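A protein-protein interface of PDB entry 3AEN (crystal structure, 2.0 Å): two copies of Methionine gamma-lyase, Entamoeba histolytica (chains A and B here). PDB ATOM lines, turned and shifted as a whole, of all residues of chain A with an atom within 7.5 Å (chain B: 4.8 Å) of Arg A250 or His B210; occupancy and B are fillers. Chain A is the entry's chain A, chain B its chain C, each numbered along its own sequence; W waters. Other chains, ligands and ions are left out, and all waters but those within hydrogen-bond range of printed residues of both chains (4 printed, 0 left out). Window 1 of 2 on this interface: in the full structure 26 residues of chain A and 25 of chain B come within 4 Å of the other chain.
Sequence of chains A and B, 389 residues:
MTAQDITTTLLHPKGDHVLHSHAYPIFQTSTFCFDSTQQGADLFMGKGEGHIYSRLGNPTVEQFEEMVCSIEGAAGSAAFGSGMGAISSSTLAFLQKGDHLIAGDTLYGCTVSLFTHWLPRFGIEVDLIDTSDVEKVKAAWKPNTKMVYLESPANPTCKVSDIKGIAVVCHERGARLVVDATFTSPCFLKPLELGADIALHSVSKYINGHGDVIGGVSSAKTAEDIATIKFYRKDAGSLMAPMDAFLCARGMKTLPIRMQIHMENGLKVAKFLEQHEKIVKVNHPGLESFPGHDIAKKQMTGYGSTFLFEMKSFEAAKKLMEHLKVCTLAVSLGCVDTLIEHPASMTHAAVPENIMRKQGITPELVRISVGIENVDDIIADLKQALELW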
ATOM      1  N   LEU A  11      22.235 -11.158 -28.568  1.00  0.00           N
ATOM      2  CA  LEU A  11      23.105 -11.629 -29.645  1.00  0.00           C
ATOM      3  C   LEU A  11      24.252 -10.641 -29.929  1.00  0.00           C
ATOM      4  O   LEU A  11      25.191 -10.980 -30.640  1.00  0.00           O
ATOM      5  CB  LEU A  11      22.265 -11.884 -30.925  1.00  0.00           C
ATOM      6  CG  LEU A  11      21.304 -13.101 -30.748  1.00  0.00           C
ATOM      7  CD1 LEU A  11      20.361 -13.271 -31.916  1.00  0.00           C
ATOM      8  CD2 LEU A  11      22.094 -14.349 -30.584  1.00  0.00           C
ATOM      9  N   HIS A  22      35.149 -14.093 -32.961  1.00  0.00           N
ATOM     10  CA  HIS A  22      33.696 -13.889 -33.038  1.00  0.00           C
ATOM     11  C   HIS A  22      32.991 -14.390 -31.758  1.00  0.00           C
ATOM     12  O   HIS A  22      32.289 -13.625 -31.093  1.00  0.00           O
ATOM     13  CB  HIS A  22      33.120 -14.553 -34.315  1.00  0.00           C
ATOM     14  CG  HIS A  22      31.643 -14.383 -34.470  1.00  0.00           C
ATOM     15  ND1 HIS A  22      30.796 -15.440 -34.721  1.00  0.00           N
ATOM     16  CD2 HIS A  22      30.857 -13.281 -34.392  1.00  0.00           C
ATOM     17  CE1 HIS A  22      29.550 -15.000 -34.790  1.00  0.00           C
ATOM     18  NE2 HIS A  22      29.556 -13.697 -34.586  1.00  0.00           N
ATOM     19  N   ALA A  23      33.189 -15.652 -31.386  1.00  0.00           N
ATOM     20  CA  ALA A  23      32.728 -16.114 -30.065  1.00  0.00           C
ATOM     21  C   ALA A  23      33.683 -15.579 -28.976  1.00  0.00           C
ATOM     22  O   ALA A  23      34.899 -15.479 -29.187  1.00  0.00           O
ATOM     23  CB  ALA A  23      32.675 -17.644 -30.004  1.00  0.00           C
ATOM     24  N   PHE A  64      28.976 -12.874 -19.435  1.00  0.00           N
ATOM     25  CA  PHE A  64      27.644 -13.419 -19.100  1.00  0.00           C
ATOM     26  C   PHE A  64      26.887 -12.450 -18.154  1.00  0.00           C
ATOM     27  O   PHE A  64      25.683 -12.179 -18.337  1.00  0.00           O
ATOM     28  CB  PHE A  64      27.765 -14.851 -18.498  1.00  0.00           C
ATOM     29  CG  PHE A  64      26.473 -15.357 -17.906  1.00  0.00           C
ATOM     30  CD1 PHE A  64      26.286 -15.337 -16.553  1.00  0.00           C
ATOM     31  CD2 PHE A  64      25.406 -15.740 -18.722  1.00  0.00           C
ATOM     32  CE1 PHE A  64      25.057 -15.716 -15.983  1.00  0.00           C
ATOM     33  CE2 PHE A  64      24.173 -16.162 -18.155  1.00  0.00           C
ATOM     34  CZ  PHE A  64      24.014 -16.169 -16.774  1.00  0.00           C
ATOM     35  N   MET A  67      25.321  -9.663 -20.045  1.00  0.00           N
ATOM     36  CA  MET A  67      24.107 -10.088 -20.747  1.00  0.00           C
ATOM     37  C   MET A  67      22.888 -10.059 -19.814  1.00  0.00           C
ATOM     38  O   MET A  67      21.828  -9.509 -20.182  1.00  0.00           O
ATOM     39  CB  MET A  67      24.248 -11.484 -21.389  1.00  0.00           C
ATOM     40  CG  MET A  67      25.367 -11.557 -22.423  1.00  0.00           C
ATOM     41  SD  MET A  67      25.580 -13.271 -22.999  1.00  0.00           S
ATOM     42  CE  MET A  67      24.009 -13.615 -23.856  1.00  0.00           C
ATOM     43  N   ILE A 207      17.514 -19.792 -17.958  1.00  0.00           N
ATOM     44  CA  ILE A 207      18.472 -18.891 -18.624  1.00  0.00           C
ATOM     45  C   ILE A 207      19.467 -19.721 -19.458  1.00  0.00           C
ATOM     46  O   ILE A 207      19.642 -19.469 -20.674  1.00  0.00           O
ATOM     47  CB  ILE A 207      19.108 -17.943 -17.602  1.00  0.00           C
ATOM     48  CG1 ILE A 207      18.024 -16.946 -17.173  1.00  0.00           C
ATOM     49  CG2 ILE A 207      20.364 -17.219 -18.214  1.00  0.00           C
ATOM     50  CD1 ILE A 207      18.378 -16.024 -15.965  1.00  0.00           C
ATOM     51  N   ASN A 208      20.068 -20.741 -18.827  1.00  0.00           N
ATOM     52  CA  ASN A 208      20.982 -21.602 -19.532  1.00  0.00           C
ATOM     53  C   ASN A 208      20.171 -22.528 -20.430  1.00  0.00           C
ATOM     54  O   ASN A 208      20.553 -22.756 -21.610  1.00  0.00           O
ATOM     55  CB  ASN A 208      21.817 -22.452 -18.573  1.00  0.00           C
ATOM     56  CG  ASN A 208      22.746 -23.396 -19.316  1.00  0.00           C
ATOM     57  OD1 ASN A 208      23.602 -22.948 -20.089  1.00  0.00           O
ATOM     58  ND2 ASN A 208      22.546 -24.713 -19.133  1.00  0.00           N
ATOM     59  N   HIS A 210      19.664 -25.677 -20.982  1.00  0.00           N
ATOM     60  CA  HIS A 210      20.107 -26.902 -21.646  1.00  0.00           C
ATOM     61  C   HIS A 210      20.424 -28.032 -20.661  1.00  0.00           C
ATOM     62  O   HIS A 210      20.959 -29.047 -21.071  1.00  0.00           O
ATOM     63  CB  HIS A 210      21.285 -26.633 -22.624  1.00  0.00           C
ATOM     64  CG  HIS A 210      20.874 -25.892 -23.859  1.00  0.00           C
ATOM     65  ND1 HIS A 210      20.540 -24.553 -23.831  1.00  0.00           N
ATOM     66  CD2 HIS A 210      20.729 -26.296 -25.151  1.00  0.00           C
ATOM     67  CE1 HIS A 210      20.209 -24.160 -25.054  1.00  0.00           C
ATOM     68  NE2 HIS A 210      20.321 -25.197 -25.876  1.00  0.00           N
ATOM     69  N   ASP A 212      22.652 -28.556 -18.479  1.00  0.00           N
ATOM     70  CA  ASP A 212      24.026 -29.023 -18.383  1.00  0.00           C
ATOM     71  C   ASP A 212      24.935 -28.130 -17.554  1.00  0.00           C
ATOM     72  O   ASP A 212      26.149 -28.321 -17.569  1.00  0.00           O
ATOM     73  CB  ASP A 212      24.609 -29.279 -19.786  1.00  0.00           C
ATOM     74  CG  ASP A 212      24.454 -28.075 -20.733  1.00  0.00           C
ATOM     75  OD1 ASP A 212      24.684 -28.246 -21.943  1.00  0.00           O
ATOM     76  OD2 ASP A 212      24.078 -26.982 -20.272  1.00  0.00           O
ATOM     77  N   ASP A 244      31.537 -22.889 -17.518  1.00  0.00           N
ATOM     78  CA  ASP A 244      30.109 -22.782 -17.279  1.00  0.00           C
ATOM     79  C   ASP A 244      29.531 -21.427 -17.741  1.00  0.00           C
ATOM     80  O   ASP A 244      28.403 -21.387 -18.238  1.00  0.00           O
ATOM     81  CB  ASP A 244      29.771 -23.044 -15.813  1.00  0.00           C
ATOM     82  CG  ASP A 244      29.830 -24.548 -15.448  1.00  0.00           C
ATOM     83  OD1 ASP A 244      29.703 -24.862 -14.234  1.00  0.00           O
ATOM     84  OD2 ASP A 244      29.998 -25.408 -16.360  1.00  0.00           O
ATOM     85  N   ALA A 245      30.280 -20.331 -17.544  1.00  0.00           N
ATOM     86  CA  ALA A 245      29.871 -19.012 -18.066  1.00  0.00           C
ATOM     87  C   ALA A 245      29.780 -19.004 -19.609  1.00  0.00           C
ATOM     88  O   ALA A 245      28.861 -18.422 -20.189  1.00  0.00           O
ATOM     89  CB  ALA A 245      30.808 -17.886 -17.580  1.00  0.00           C
ATOM     90  N   PHE A 246      30.748 -19.630 -20.271  1.00  0.00           N
ATOM     91  CA  PHE A 246      30.677 -19.807 -21.734  1.00  0.00           C
ATOM     92  C   PHE A 246      29.367 -20.535 -22.115  1.00  0.00           C
ATOM     93  O   PHE A 246      28.651 -20.111 -23.039  1.00  0.00           O
ATOM     94  CB  PHE A 246      31.884 -20.621 -22.207  1.00  0.00           C
ATOM     95  CG  PHE A 246      31.751 -21.169 -23.602  1.00  0.00           C
ATOM     96  CD1 PHE A 246      32.107 -20.377 -24.721  1.00  0.00           C
ATOM     97  CD2 PHE A 246      31.318 -22.496 -23.803  1.00  0.00           C
ATOM     98  CE1 PHE A 246      32.010 -20.893 -26.015  1.00  0.00           C
ATOM     99  CE2 PHE A 246      31.225 -23.020 -25.069  1.00  0.00           C
ATOM    100  CZ  PHE A 246      31.557 -22.226 -26.184  1.00  0.00           C
ATOM    101  N   LEU A 247      29.059 -21.629 -21.427  1.00  0.00           N
ATOM    102  CA  LEU A 247      27.820 -22.397 -21.737  1.00  0.00           C
ATOM    103  C   LEU A 247      26.564 -21.596 -21.417  1.00  0.00           C
ATOM    104  O   LEU A 247      25.622 -21.655 -22.179  1.00  0.00           O
ATOM    105  CB  LEU A 247      27.773 -23.763 -20.981  1.00  0.00           C
ATOM    106  CG  LEU A 247      28.862 -24.767 -21.427  1.00  0.00           C
ATOM    107  CD1 LEU A 247      28.971 -26.003 -20.453  1.00  0.00           C
ATOM    108  CD2 LEU A 247      28.621 -25.255 -22.884  1.00  0.00           C
ATOM    109  N   CYS A 248      26.525 -20.874 -20.286  1.00  0.00           N
ATOM    110  CA  CYS A 248      25.329 -20.065 -19.950  1.00  0.00           C
ATOM    111  C   CYS A 248      25.092 -18.948 -20.941  1.00  0.00           C
ATOM    112  O   CYS A 248      23.928 -18.708 -21.335  1.00  0.00           O
ATOM    113  CB  CYS A 248      25.368 -19.497 -18.521  1.00  0.00           C
ATOM    114  SG  CYS A 248      25.377 -20.807 -17.277  1.00  0.00           S
ATOM    115  N   ALA A 249      26.157 -18.256 -21.342  1.00  0.00           N
ATOM    116  CA  ALA A 249      26.031 -17.175 -22.376  1.00  0.00           C
ATOM    117  C   ALA A 249      25.527 -17.748 -23.693  1.00  0.00           C
ATOM    118  O   ALA A 249      24.653 -17.163 -24.337  1.00  0.00           O
ATOM    119  CB  ALA A 249      27.367 -16.429 -22.594  1.00  0.00           C
ATOM    120  N   ARG A 250      26.072 -18.897 -24.070  1.00  0.00           N
ATOM    121  CA  ARG A 250      25.633 -19.636 -25.245  1.00  0.00           C
ATOM    122  C   ARG A 250      24.129 -20.049 -25.158  1.00  0.00           C
ATOM    123  O   ARG A 250      23.352 -19.827 -26.110  1.00  0.00           O
ATOM    124  CB  ARG A 250      26.456 -20.918 -25.373  1.00  0.00           C
ATOM    125  CG  ARG A 250      26.237 -21.654 -26.724  1.00  0.00           C
ATOM    126  CD  ARG A 250      27.056 -22.936 -26.667  1.00  0.00           C
ATOM    127  NE  ARG A 250      27.492 -23.475 -27.971  1.00  0.00           N
ATOM    128  CZ  ARG A 250      26.985 -24.529 -28.600  1.00  0.00           C
ATOM    129  NH1 ARG A 250      27.583 -24.949 -29.711  1.00  0.00           N
ATOM    130  NH2 ARG A 250      25.913 -25.190 -28.139  1.00  0.00           N
ATOM    131  N   GLY A 251      23.727 -20.628 -24.039  1.00  0.00           N
ATOM    132  CA  GLY A 251      22.305 -20.989 -23.849  1.00  0.00           C
ATOM    133  C   GLY A 251      21.415 -19.756 -23.887  1.00  0.00           C
ATOM    134  O   GLY A 251      20.353 -19.737 -24.503  1.00  0.00           O
ATOM    135  N   MET A 252      21.893 -18.695 -23.272  1.00  0.00           N
ATOM    136  CA  MET A 252      21.153 -17.452 -23.242  1.00  0.00           C
ATOM    137  C   MET A 252      20.950 -16.808 -24.631  1.00  0.00           C
ATOM    138  O   MET A 252      20.008 -16.057 -24.811  1.00  0.00           O
ATOM    139  CB  MET A 252      21.823 -16.464 -22.288  1.00  0.00           C
ATOM    140  CG  MET A 252      20.886 -15.338 -21.858  1.00  0.00           C
ATOM    141  SD  MET A 252      21.615 -14.332 -20.545  1.00  0.00           S
ATOM    142  CE  MET A 252      20.138 -13.382 -20.215  1.00  0.00           C
ATOM    143  N   LYS A 253      21.779 -17.157 -25.614  1.00  0.00           N
ATOM    144  CA  LYS A 253      21.587 -16.612 -26.995  1.00  0.00           C
ATOM    145  C   LYS A 253      20.214 -16.972 -27.580  1.00  0.00           C
ATOM    146  O   LYS A 253      19.711 -16.253 -28.448  1.00  0.00           O
ATOM    147  CB  LYS A 253      22.671 -17.092 -27.976  1.00  0.00           C
ATOM    148  CG  LYS A 253      24.101 -16.708 -27.619  1.00  0.00           C
ATOM    149  CD  LYS A 253      24.241 -15.245 -27.386  1.00  0.00           C
ATOM    150  CE  LYS A 253      25.735 -14.824 -27.354  1.00  0.00           C
ATOM    151  NZ  LYS A 253      25.817 -13.336 -27.301  1.00  0.00           N
ATOM    152  N   THR A 254      19.639 -18.083 -27.125  1.00  0.00           N
ATOM    153  CA  THR A 254      18.292 -18.542 -27.569  1.00  0.00           C
ATOM    154  C   THR A 254      17.211 -18.373 -26.515  1.00  0.00           C
ATOM    155  O   THR A 254      16.121 -18.907 -26.655  1.00  0.00           O
ATOM    156  CB  THR A 254      18.250 -20.024 -28.020  1.00  0.00           C
ATOM    157  OG1 THR A 254      18.827 -20.889 -27.008  1.00  0.00           O
ATOM    158  CG2 THR A 254      19.016 -20.181 -29.387  1.00  0.00           C
ATOM    159  N   LEU A 255      17.500 -17.655 -25.454  1.00  0.00           N
ATOM    160  CA  LEU A 255      16.518 -17.562 -24.382  1.00  0.00           C
ATOM    161  C   LEU A 255      15.167 -16.987 -24.866  1.00  0.00           C
ATOM    162  O   LEU A 255      14.145 -17.582 -24.572  1.00  0.00           O
ATOM    163  CB  LEU A 255      17.050 -16.756 -23.159  1.00  0.00           C
ATOM    164  CG  LEU A 255      16.056 -16.540 -21.993  1.00  0.00           C
ATOM    165  CD1 LEU A 255      15.675 -17.902 -21.341  1.00  0.00           C
ATOM    166  CD2 LEU A 255      16.595 -15.539 -20.912  1.00  0.00           C
ATOM    167  N   ARG A 258      13.309 -19.600 -26.956  1.00  0.00           N
ATOM    168  CA  ARG A 258      12.923 -20.730 -26.094  1.00  0.00           C
ATOM    169  C   ARG A 258      11.754 -20.344 -25.174  1.00  0.00           C
ATOM    170  O   ARG A 258      10.772 -21.099 -25.059  1.00  0.00           O
ATOM    171  CB  ARG A 258      14.091 -21.279 -25.265  1.00  0.00           C
ATOM    172  CG  ARG A 258      15.155 -22.003 -26.123  1.00  0.00           C
ATOM    173  CD  ARG A 258      16.301 -22.563 -25.245  1.00  0.00           C
ATOM    174  NE  ARG A 258      17.195 -21.526 -24.669  1.00  0.00           N
ATOM    175  CZ  ARG A 258      17.175 -21.119 -23.390  1.00  0.00           C
ATOM    176  NH1 ARG A 258      16.270 -21.619 -22.527  1.00  0.00           N
ATOM    177  NH2 ARG A 258      18.089 -20.248 -22.953  1.00  0.00           N
ATOM    178  N   ASN B 208      25.318 -26.792 -35.715  1.00  0.00           N
ATOM    179  CA  ASN B 208      25.778 -26.386 -34.404  1.00  0.00           C
ATOM    180  C   ASN B 208      25.156 -25.026 -34.093  1.00  0.00           C
ATOM    181  O   ASN B 208      24.643 -24.782 -32.976  1.00  0.00           O
ATOM    182  CB  ASN B 208      27.307 -26.256 -34.353  1.00  0.00           C
ATOM    183  CG  ASN B 208      27.775 -25.759 -33.019  1.00  0.00           C
ATOM    184  OD1 ASN B 208      27.523 -26.399 -31.994  1.00  0.00           O
ATOM    185  ND2 ASN B 208      28.437 -24.596 -33.003  1.00  0.00           N
ATOM    186  N   GLY B 209      25.243 -24.124 -35.082  1.00  0.00           N
ATOM    187  CA  GLY B 209      24.551 -22.852 -35.058  1.00  0.00           C
ATOM    188  C   GLY B 209      25.076 -21.717 -34.174  1.00  0.00           C
ATOM    189  O   GLY B 209      24.540 -20.611 -34.238  1.00  0.00           O
ATOM    190  N   HIS B 210      26.088 -21.984 -33.340  1.00  0.00           N
ATOM    191  CA  HIS B 210      26.479 -21.007 -32.341  1.00  0.00           C
ATOM    192  C   HIS B 210      27.875 -20.420 -32.614  1.00  0.00           C
ATOM    193  O   HIS B 210      28.413 -19.728 -31.768  1.00  0.00           O
ATOM    194  CB  HIS B 210      26.363 -21.599 -30.920  1.00  0.00           C
ATOM    195  CG  HIS B 210      24.940 -21.768 -30.456  1.00  0.00           C
ATOM    196  ND1 HIS B 210      24.092 -22.701 -31.010  1.00  0.00           N
ATOM    197  CD2 HIS B 210      24.210 -21.096 -29.527  1.00  0.00           C
ATOM    198  CE1 HIS B 210      22.904 -22.620 -30.427  1.00  0.00           C
ATOM    199  NE2 HIS B 210      22.954 -21.669 -29.509  1.00  0.00           N
ATOM    200  N   GLY B 211      28.444 -20.723 -33.788  1.00  0.00           N
ATOM    201  CA  GLY B 211      29.719 -20.083 -34.238  1.00  0.00           C
ATOM    202  C   GLY B 211      30.883 -20.430 -33.331  1.00  0.00           C
ATOM    203  O   GLY B 211      31.866 -19.715 -33.260  1.00  0.00           O
ATOM    204  N   ASP B 212      30.800 -21.554 -32.635  1.00  0.00           N
ATOM    205  CA  ASP B 212      31.870 -21.840 -31.698  1.00  0.00           C
ATOM    206  C   ASP B 212      32.501 -23.202 -31.883  1.00  0.00           C
ATOM    207  O   ASP B 212      33.286 -23.603 -31.052  1.00  0.00           O
ATOM    208  CB  ASP B 212      31.400 -21.616 -30.248  1.00  0.00           C
ATOM    209  CG  ASP B 212      30.117 -22.374 -29.922  1.00  0.00           C
ATOM    210  OD1 ASP B 212      29.528 -22.112 -28.854  1.00  0.00           O
ATOM    211  OD2 ASP B 212      29.706 -23.239 -30.728  1.00  0.00           O
ATOM    212  N   VAL B 213      32.106 -23.950 -32.921  1.00  0.00           N
ATOM    213  CA  VAL B 213      32.820 -25.185 -33.246  1.00  0.00           C
ATOM    214  C   VAL B 213      32.977 -25.347 -34.756  1.00  0.00           C
ATOM    215  O   VAL B 213      32.135 -24.880 -35.544  1.00  0.00           O
ATOM    216  CB  VAL B 213      32.304 -26.531 -32.499  1.00  0.00           C
ATOM    217  CG1 VAL B 213      31.215 -26.316 -31.447  1.00  0.00           C
ATOM    218  CG2 VAL B 213      32.096 -27.706 -33.399  1.00  0.00           C
ATOM    219  N   LEU B 247      29.099 -29.969 -27.674  1.00  0.00           N
ATOM    220  CA  LEU B 247      28.608 -28.657 -28.177  1.00  0.00           C
ATOM    221  C   LEU B 247      27.685 -28.745 -29.390  1.00  0.00           C
ATOM    222  O   LEU B 247      26.668 -28.059 -29.432  1.00  0.00           O
ATOM    223  CB  LEU B 247      29.791 -27.701 -28.461  1.00  0.00           C
ATOM    224  CG  LEU B 247      30.550 -27.208 -27.209  1.00  0.00           C
ATOM    225  CD1 LEU B 247      31.800 -26.366 -27.647  1.00  0.00           C
ATOM    226  CD2 LEU B 247      29.660 -26.401 -26.224  1.00  0.00           C
ATOM    227  N   CYS B 248      28.035 -29.593 -30.372  1.00  0.00           N
ATOM    228  CA  CYS B 248      27.204 -29.780 -31.570  1.00  0.00           C
ATOM    229  C   CYS B 248      25.860 -30.418 -31.245  1.00  0.00           C
ATOM    230  O   CYS B 248      24.830 -29.952 -31.750  1.00  0.00           O
ATOM    231  CB  CYS B 248      27.922 -30.620 -32.652  1.00  0.00           C
ATOM    232  SG  CYS B 248      29.338 -29.720 -33.321  1.00  0.00           S
ATOM    233  N   ARG B 250      24.338 -30.234 -28.396  1.00  0.00           N
ATOM    234  CA  ARG B 250      23.631 -29.171 -27.664  1.00  0.00           C
ATOM    235  C   ARG B 250      23.042 -28.094 -28.624  1.00  0.00           C
ATOM    236  O   ARG B 250      21.874 -27.677 -28.474  1.00  0.00           O
ATOM    237  CB  ARG B 250      24.619 -28.491 -26.698  1.00  0.00           C
ATOM    238  CG  ARG B 250      23.967 -27.514 -25.754  1.00  0.00           C
ATOM    239  CD  ARG B 250      25.057 -26.714 -25.077  1.00  0.00           C
ATOM    240  NE  ARG B 250      24.776 -26.265 -23.713  1.00  0.00           N
ATOM    241  CZ  ARG B 250      24.622 -24.996 -23.335  1.00  0.00           C
ATOM    242  NH1 ARG B 250      24.496 -24.716 -22.045  1.00  0.00           N
ATOM    243  NH2 ARG B 250      24.645 -23.992 -24.226  1.00  0.00           N
ATOM    244  N   GLY B 251      23.857 -27.621 -29.562  1.00  0.00           N
ATOM    245  CA  GLY B 251      23.385 -26.667 -30.583  1.00  0.00           C
ATOM    246  C   GLY B 251      22.202 -27.245 -31.356  1.00  0.00           C
ATOM    247  O   GLY B 251      21.199 -26.569 -31.619  1.00  0.00           O
ATOM    248  N   THR B 254      18.233 -27.054 -30.498  1.00  0.00           N
ATOM    249  CA  THR B 254      17.428 -25.891 -30.981  1.00  0.00           C
ATOM    250  C   THR B 254      17.425 -25.722 -32.489  1.00  0.00           C
ATOM    251  O   THR B 254      16.903 -24.723 -32.990  1.00  0.00           O
ATOM    252  CB  THR B 254      17.838 -24.531 -30.347  1.00  0.00           C
ATOM    253  OG1 THR B 254      19.252 -24.274 -30.583  1.00  0.00           O
ATOM    254  CG2 THR B 254      17.532 -24.559 -28.806  1.00  0.00           C
ATOM    255  N   ARG B 258      15.502 -22.663 -34.549  1.00  0.00           N
ATOM    256  CA  ARG B 258      16.423 -21.678 -35.140  1.00  0.00           C
ATOM    257  C   ARG B 258      16.185 -21.609 -36.672  1.00  0.00           C
ATOM    258  O   ARG B 258      16.054 -20.493 -37.255  1.00  0.00           O
ATOM    259  CB  ARG B 258      17.885 -22.050 -34.843  1.00  0.00           C
ATOM    260  CG  ARG B 258      18.336 -21.699 -33.404  1.00  0.00           C
ATOM    261  CD  ARG B 258      19.834 -22.018 -33.188  1.00  0.00           C
ATOM    262  NE  ARG B 258      20.187 -23.459 -33.242  1.00  0.00           N
ATOM    263  CZ  ARG B 258      20.788 -24.060 -34.282  1.00  0.00           C
ATOM    264  NH1 ARG B 258      21.078 -23.380 -35.392  1.00  0.00           N
ATOM    265  NH2 ARG B 258      21.103 -25.344 -34.211  1.00  0.00           N
ATOM    266  N   VAL B 336      23.718 -17.868 -35.013  1.00  0.00           N
ATOM    267  CA  VAL B 336      22.542 -17.192 -34.458  1.00  0.00           C
ATOM    268  C   VAL B 336      22.566 -15.696 -34.784  1.00  0.00           C
ATOM    269  O   VAL B 336      21.515 -15.076 -34.942  1.00  0.00           O
ATOM    270  CB  VAL B 336      22.412 -17.421 -32.931  1.00  0.00           C
ATOM    271  CG1 VAL B 336      21.915 -18.819 -32.634  1.00  0.00           C
ATOM    272  CG2 VAL B 336      23.752 -17.169 -32.226  1.00  0.00           C
HETATM  273  O   HOH W   1      21.467 -21.406 -27.172  1.00  0.00           O
HETATM  274  O   HOH W   2      23.283 -23.930 -27.053  1.00  0.00           O
HETATM  275  O   HOH W   3      20.885 -25.190 -28.543  1.00  0.00           O
HETATM  276  O   HOH W   4      32.231 -17.840 -35.124  1.00  0.00           O
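OD1 of Asn A208 sits at hydrogen-bond distance from NH1 of Arg B250 (2.8 Å). OD1 of Asp A212 is in salt-bridge range of NE of Arg B250 (2.7 Å). The backbone carbonyl oxygen (O) of Leu A247 is in hydrogen-bond range of the guanidinium group (NH2) of Arg B250 (3.3 Å). The side-chain amide oxygen of Asn B208 lies within hydrogen-bond range of the guanidinium group of Arg A250, 2.7 Å away. NE of Arg A250 lies within salt-bridge range of OD1 of Asp B212. O of Leu B247 sits at hydrogen-bond distance from NH2 of Arg A250, 3.2 Å away. NH2 of Arg A250 lies close to N of Gly B251 (3.5 Å). The guanidinium group (NH2) of Arg B250 sits close to the backbone NH (N) of Gly A251 (3.5 Å).
The backbone carbonyl oxygen of Asn A208 lies within hydrogen-bond range of a ring nitrogen (ND1) of His A210 (2.9 Å). O of Asn B208 is in hydrogen-bond range of ND1 of His B210 (2.9 Å). The side-chain amide nitrogen (ND2) of Asn B208 is in hydrogen-bond range of the side-chain carboxylate (OD2) of Asp B212 (2.9 Å). O of Gly B209 sits at hydrogen-bond distance from N of Val B336, at 3.0 Å. O of Gly B251 lies within hydrogen-bond range of OG1 of Thr B254 (3.2 Å). The backbone carbonyl oxygen of Gly B251 lies within hydrogen-bond range of the guanidinium group of Arg B258, 2.9 Å away.
Leu A11 touches Val B336 (CD2 to CG2, 3.7 Å). Gly B211 touches Ala A23 (O to CB, 3.9 Å). CD2 of His A210 touches CG of Arg B250 (3.5 Å). CZ of Phe A246 touches OD1 of Asp B212, at 3.4 Å. CE2 of Phe A246 touches CD2 of Leu B247 (3.9 Å). Leu A247 touches Leu B247. Arg A250 touches His B210 (CG to CD2, 3.5 Å). NH2 of Arg A250 touches CD of Arg B250, 3.5 Å away.
Arg A250 touches six residues of chain B. Of chain A, only Arg A250 (3.5 Å) comes within 4 Å of His B210. No residue of chain A comes within 4 Å of Gly B209. Of the printed residues of chain B, Gly A251 touches Arg B250 (3.5 Å). Printed residues of chain A within 4 Å of Gly B251: Arg A250. Of the printed residues of chain A, Asn B208 touches Arg A250 (2.7 Å). Of the printed residues of chain B, Phe A246 touches Asp B212 and Leu B247. Of the printed residues of chain B, Leu A11 touches Val B336. The nearest printed residue of chain B that does not touch Asp A212 is Leu B247 (6.8 Å).
Printed residues of chain A that touch a printed residue of chain B: Leu A11, Ala A23, Asn A208, His A210, Asp A212, Phe A246, Leu A247, Arg A250 and Gly A251. Hydrophobic or aromatic side chains of chain A that line the printed part of chain B: Leu A11, Ala A23, His A210, Phe A246 and Leu A247. Among the printed residues, Asp or Glu carboxylates within 4 Å of a Lys or Arg side-chain nitrogen of the other chain: Asp A212 with Arg B250 and Arg A250 with Asp B212.
Asn A208 touches Arg B250, and with the chains exchanged Arg A250 touches Asn B208. His A210 touches Arg B250, and with the chains exchanged Arg A250 touches His B210. Arg A250 touches its own counterpart, Arg B250. Arg A250 touches Gly B251, and with the chains exchanged Gly A251 touches Arg B250. Positions printed for both chains: 208, 210, 212, 247, 248, 250, 251, 254 and 258.
Water W4 lies within hydrogen-bond range of O of Gly B211 (2.7 Å) and ND1 of His A22 (2.8 Å). Water W3 lies within hydrogen-bond range of O of Arg B250 (2.7 Å), NE2 of His A210 (2.7 Å), OG1 of Thr B254 (2.8 Å) and O of Gly B251 (3.4 Å). Water W1 lies within hydrogen-bond range of O of Arg A250, OG1 of Thr A254, NE2 of His B210 and O of Gly A251. Water W2 lies within hydrogen-bond range of the guanidinium group of Arg A250 (3.1 Å), the guanidinium group of Arg B250 (3.1 Å), a ring nitrogen (NE2) of His B210 (3.4 Å) and a ring nitrogen (NE2) of His A210 (3.4 Å).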
